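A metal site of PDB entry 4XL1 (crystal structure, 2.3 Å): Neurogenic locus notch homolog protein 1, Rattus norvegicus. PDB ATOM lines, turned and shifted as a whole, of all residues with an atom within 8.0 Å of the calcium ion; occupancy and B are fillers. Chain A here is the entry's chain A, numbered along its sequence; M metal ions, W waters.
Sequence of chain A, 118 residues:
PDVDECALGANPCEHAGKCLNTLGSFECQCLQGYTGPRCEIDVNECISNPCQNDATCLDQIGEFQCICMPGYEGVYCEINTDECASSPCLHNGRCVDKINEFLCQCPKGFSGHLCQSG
Within 4 Å of the calcium ion: Asn 80, Thr 81, Glu 83, Asp 97 and Lys 98.
OE2 of Glu 83 sits close to N of Asn 100 (3.4 Å).
N of Thr 81 lies within hydrogen-bond range of O of Gly 71 (3.0 Å).
The backbone NH (N) of Asp 97 sits at hydrogen-bond distance from the side-chain sulfur (SG) of Cys 84.
OE1 of Glu 83 binds the calcium ion, 2.4 Å away.
The side-chain amide oxygen (OD1) of Asn 80 binds the calcium ion (2.4 Å).
The calcium ion is bound by O of Thr 81 (2.4 Å).
O of Lys 98 binds the calcium ion (2.4 Å).
The calcium ion is bound by water W1 (2.4 Å).
OD1 of Asp 97 is bound to the calcium ion (2.4 Å).
Water W2 is bound to the calcium ion, at 2.4 Å.
OD2 of Asp 97 is bound to the calcium ion, at 2.4 Å.
Water W2 lies within hydrogen-bond range of the side-chain carboxylate (OE2) of Glu 83 (2.5 Å), the backbone NH (N) of Asn 100 (2.9 Å) and the backbone carbonyl oxygen (O) of Gly 71 (3.0 Å).
Water W1 bridges the side-chain amide nitrogen (ND2) of Asn 80 and the backbone carbonyl oxygen (O) of Asp 97.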
ATOM      1  N   PRO A  70      -6.316 -33.798  20.689  1.00  0.00           N
ATOM      2  CA  PRO A  70      -7.744 -33.669  21.003  1.00  0.00           C
ATOM      3  C   PRO A  70      -8.120 -32.253  21.398  1.00  0.00           C
ATOM      4  O   PRO A  70      -7.437 -31.639  22.221  1.00  0.00           O
ATOM      5  CB  PRO A  70      -7.928 -34.643  22.168  1.00  0.00           C
ATOM      6  CG  PRO A  70      -6.867 -35.675  21.961  1.00  0.00           C
ATOM      7  CD  PRO A  70      -5.690 -34.921  21.404  1.00  0.00           C
ATOM      8  N   GLY A  71      -9.206 -31.732  20.822  1.00  0.00           N
ATOM      9  CA  GLY A  71      -9.645 -30.378  21.092  1.00  0.00           C
ATOM     10  C   GLY A  71      -9.239 -29.351  20.053  1.00  0.00           C
ATOM     11  O   GLY A  71      -9.587 -28.177  20.170  1.00  0.00           O
ATOM     12  N   TYR A  72      -8.498 -29.781  19.041  1.00  0.00           N
ATOM     13  CA  TYR A  72      -8.074 -28.867  17.981  1.00  0.00           C
ATOM     14  C   TYR A  72      -8.628 -29.318  16.636  1.00  0.00           C
ATOM     15  O   TYR A  72      -8.950 -30.484  16.440  1.00  0.00           O
ATOM     16  CB  TYR A  72      -6.554 -28.776  17.912  1.00  0.00           C
ATOM     17  CG  TYR A  72      -5.927 -28.177  19.150  1.00  0.00           C
ATOM     18  CD1 TYR A  72      -5.634 -28.969  20.248  1.00  0.00           C
ATOM     19  CD2 TYR A  72      -5.662 -26.808  19.235  1.00  0.00           C
ATOM     20  CE1 TYR A  72      -5.070 -28.438  21.382  1.00  0.00           C
ATOM     21  CE2 TYR A  72      -5.099 -26.263  20.368  1.00  0.00           C
ATOM     22  CZ  TYR A  72      -4.811 -27.085  21.445  1.00  0.00           C
ATOM     23  OH  TYR A  72      -4.250 -26.554  22.589  1.00  0.00           O
ATOM     24  N   ILE A  79      -7.029 -24.201  14.964  1.00  0.00           N
ATOM     25  CA  ILE A  79      -8.253 -23.787  15.634  1.00  0.00           C
ATOM     26  C   ILE A  79      -8.505 -24.589  16.907  1.00  0.00           C
ATOM     27  O   ILE A  79      -8.516 -25.813  16.892  1.00  0.00           O
ATOM     28  CB  ILE A  79      -9.486 -23.915  14.724  1.00  0.00           C
ATOM     29  CG1 ILE A  79      -9.296 -23.089  13.450  1.00  0.00           C
ATOM     30  CG2 ILE A  79     -10.735 -23.456  15.457  1.00  0.00           C
ATOM     31  CD1 ILE A  79     -10.347 -23.355  12.395  1.00  0.00           C
ATOM     32  N   ASN A  80      -8.705 -23.870  18.008  1.00  0.00           N
ATOM     33  CA  ASN A  80      -9.150 -24.461  19.261  1.00  0.00           C
ATOM     34  C   ASN A  80     -10.673 -24.572  19.256  1.00  0.00           C
ATOM     35  O   ASN A  80     -11.366 -23.560  19.240  1.00  0.00           O
ATOM     36  CB  ASN A  80      -8.666 -23.620  20.453  1.00  0.00           C
ATOM     37  CG  ASN A  80      -8.952 -24.257  21.804  1.00  0.00           C
ATOM     38  OD1 ASN A  80      -9.950 -24.948  21.986  1.00  0.00           O
ATOM     39  ND2 ASN A  80      -8.058 -24.024  22.754  1.00  0.00           N
ATOM     40  N   THR A  81     -11.185 -25.799  19.241  1.00  0.00           N
ATOM     41  CA  THR A  81     -12.623 -26.027  19.173  1.00  0.00           C
ATOM     42  C   THR A  81     -13.352 -25.415  20.363  1.00  0.00           C
ATOM     43  O   THR A  81     -12.981 -25.644  21.511  1.00  0.00           O
ATOM     44  CB  THR A  81     -12.968 -27.529  19.097  1.00  0.00           C
ATOM     45  OG1 THR A  81     -12.327 -28.124  17.961  1.00  0.00           O
ATOM     46  CG2 THR A  81     -14.469 -27.737  18.986  1.00  0.00           C
ATOM     47  N   ASP A  82     -14.383 -24.631  20.082  1.00  0.00           N
ATOM     48  CA  ASP A  82     -15.151 -23.966  21.130  1.00  0.00           C
ATOM     49  C   ASP A  82     -16.231 -24.906  21.652  1.00  0.00           C
ATOM     50  O   ASP A  82     -17.298 -25.031  21.052  1.00  0.00           O
ATOM     51  CB  ASP A  82     -15.784 -22.661  20.607  1.00  0.00           C
ATOM     52  CG  ASP A  82     -16.495 -21.869  21.691  1.00  0.00           C
ATOM     53  OD1 ASP A  82     -16.583 -22.346  22.850  1.00  0.00           O
ATOM     54  OD2 ASP A  82     -16.973 -20.752  21.385  1.00  0.00           O
ATOM     55  N   GLU A  83     -15.952 -25.549  22.772  1.00  0.00           N
ATOM     56  CA  GLU A  83     -16.875 -26.523  23.348  1.00  0.00           C
ATOM     57  C   GLU A  83     -18.116 -25.857  23.951  1.00  0.00           C
ATOM     58  O   GLU A  83     -19.088 -26.538  24.278  1.00  0.00           O
ATOM     59  CB  GLU A  83     -16.160 -27.370  24.412  1.00  0.00           C
ATOM     60  CG  GLU A  83     -15.297 -28.482  23.834  1.00  0.00           C
ATOM     61  CD  GLU A  83     -13.898 -28.013  23.457  1.00  0.00           C
ATOM     62  OE1 GLU A  83     -13.499 -26.912  23.893  1.00  0.00           O
ATOM     63  OE2 GLU A  83     -13.206 -28.743  22.724  1.00  0.00           O
ATOM     64  N   CYS A  84     -18.073 -24.537  24.110  1.00  0.00           N
ATOM     65  CA  CYS A  84     -19.203 -23.795  24.674  1.00  0.00           C
ATOM     66  C   CYS A  84     -20.107 -23.139  23.627  1.00  0.00           C
ATOM     67  O   CYS A  84     -21.009 -22.371  23.971  1.00  0.00           O
ATOM     68  CB  CYS A  84     -18.695 -22.710  25.633  1.00  0.00           C
ATOM     69  SG  CYS A  84     -17.888 -23.354  27.122  1.00  0.00           S
ATOM     70  N   VAL A  96     -17.090 -22.675  30.528  1.00  0.00           N
ATOM     71  CA  VAL A  96     -15.684 -22.352  30.307  1.00  0.00           C
ATOM     72  C   VAL A  96     -15.089 -23.279  29.251  1.00  0.00           C
ATOM     73  O   VAL A  96     -15.014 -24.491  29.445  1.00  0.00           O
ATOM     74  CB  VAL A  96     -14.872 -22.488  31.611  1.00  0.00           C
ATOM     75  CG1 VAL A  96     -13.480 -21.894  31.440  1.00  0.00           C
ATOM     76  CG2 VAL A  96     -15.590 -21.813  32.771  1.00  0.00           C
ATOM     77  N   ASP A  97     -14.657 -22.710  28.132  1.00  0.00           N
ATOM     78  CA  ASP A  97     -14.076 -23.504  27.056  1.00  0.00           C
ATOM     79  C   ASP A  97     -12.677 -23.978  27.420  1.00  0.00           C
ATOM     80  O   ASP A  97     -11.785 -23.171  27.653  1.00  0.00           O
ATOM     81  CB  ASP A  97     -14.020 -22.733  25.750  1.00  0.00           C
ATOM     82  CG  ASP A  97     -13.418 -23.558  24.619  1.00  0.00           C
ATOM     83  OD1 ASP A  97     -13.884 -24.694  24.395  1.00  0.00           O
ATOM     84  OD2 ASP A  97     -12.463 -23.075  23.976  1.00  0.00           O
ATOM     85  N   LYS A  98     -12.502 -25.298  27.461  1.00  0.00           N
ATOM     86  CA  LYS A  98     -11.199 -25.867  27.785  1.00  0.00           C
ATOM     87  C   LYS A  98     -10.672 -26.686  26.607  1.00  0.00           C
ATOM     88  O   LYS A  98     -11.176 -26.593  25.493  1.00  0.00           O
ATOM     89  CB  LYS A  98     -11.301 -26.708  29.047  1.00  0.00           C
ATOM     90  CG  LYS A  98     -11.618 -25.876  30.284  1.00  0.00           C
ATOM     91  CD  LYS A  98     -11.554 -26.697  31.559  1.00  0.00           C
ATOM     92  CE  LYS A  98     -10.179 -26.603  32.191  1.00  0.00           C
ATOM     93  NZ  LYS A  98     -10.050 -27.516  33.365  1.00  0.00           N
ATOM     94  N   ILE A  99      -9.653 -27.500  26.886  1.00  0.00           N
ATOM     95  CA  ILE A  99      -9.029 -28.325  25.847  1.00  0.00           C
ATOM     96  C   ILE A  99      -9.791 -29.638  25.665  1.00  0.00           C
ATOM     97  O   ILE A  99      -9.734 -30.512  26.528  1.00  0.00           O
ATOM     98  CB  ILE A  99      -7.566 -28.624  26.195  1.00  0.00           C
ATOM     99  CG1 ILE A  99      -6.842 -27.330  26.586  1.00  0.00           C
ATOM    100  CG2 ILE A  99      -6.874 -29.316  25.026  1.00  0.00           C
ATOM    101  CD1 ILE A  99      -6.564 -26.405  25.423  1.00  0.00           C
ATOM    102  N   ASN A 100     -10.542 -29.719  24.579  1.00  0.00           N
ATOM    103  CA  ASN A 100     -11.405 -30.850  24.241  1.00  0.00           C
ATOM    104  C   ASN A 100     -12.439 -31.085  25.314  1.00  0.00           C
ATOM    105  O   ASN A 100     -12.913 -32.191  25.487  1.00  0.00           O
ATOM    106  CB  ASN A 100     -10.619 -32.133  23.991  1.00  0.00           C
ATOM    107  CG  ASN A 100     -11.402 -33.143  23.200  1.00  0.00           C
ATOM    108  OD1 ASN A 100     -11.801 -32.886  22.084  1.00  0.00           O
ATOM    109  ND2 ASN A 100     -11.636 -34.277  23.783  1.00  0.00           N
ATOM    110  N   GLU A 101     -12.755 -30.014  26.036  1.00  0.00           N
ATOM    111  CA  GLU A 101     -13.632 -30.055  27.188  1.00  0.00           C
ATOM    112  C   GLU A 101     -14.352 -28.721  27.384  1.00  0.00           C
ATOM    113  O   GLU A 101     -14.018 -27.717  26.745  1.00  0.00           O
ATOM    114  CB  GLU A 101     -12.855 -30.402  28.456  1.00  0.00           C
ATOM    115  CG  GLU A 101     -12.804 -31.877  28.798  1.00  0.00           C
ATOM    116  CD  GLU A 101     -12.043 -32.110  30.079  1.00  0.00           C
ATOM    117  OE1 GLU A 101     -11.473 -31.131  30.619  1.00  0.00           O
ATOM    118  OE2 GLU A 101     -12.014 -33.259  30.550  1.00  0.00           O
ATOM    119  N   PHE A 102     -15.316 -28.726  28.294  1.00  0.00           N
ATOM    120  CA  PHE A 102     -16.069 -27.539  28.674  1.00  0.00           C
ATOM    121  C   PHE A 102     -16.469 -27.667  30.127  1.00  0.00           C
ATOM    122  O   PHE A 102     -17.004 -28.689  30.478  1.00  0.00           O
ATOM    123  CB  PHE A 102     -17.278 -27.316  27.792  1.00  0.00           C
ATOM    124  CG  PHE A 102     -18.469 -28.140  28.145  1.00  0.00           C
ATOM    125  CD1 PHE A 102     -19.237 -27.835  29.227  1.00  0.00           C
ATOM    126  CD2 PHE A 102     -18.856 -29.205  27.353  1.00  0.00           C
ATOM    127  CE1 PHE A 102     -20.340 -28.563  29.533  1.00  0.00           C
ATOM    128  CE2 PHE A 102     -19.957 -29.961  27.661  1.00  0.00           C
ATOM    129  CZ  PHE A 102     -20.706 -29.633  28.748  1.00  0.00           C
HETATM  130 CA    CA M   1     -11.728 -25.362  23.521  1.00  0.00          CA
HETATM  131  O   HOH W   1     -10.362 -23.905  24.853  1.00  0.00           O
HETATM  132  O   HOH W   2     -10.986 -27.515  22.695  1.00  0.00           O
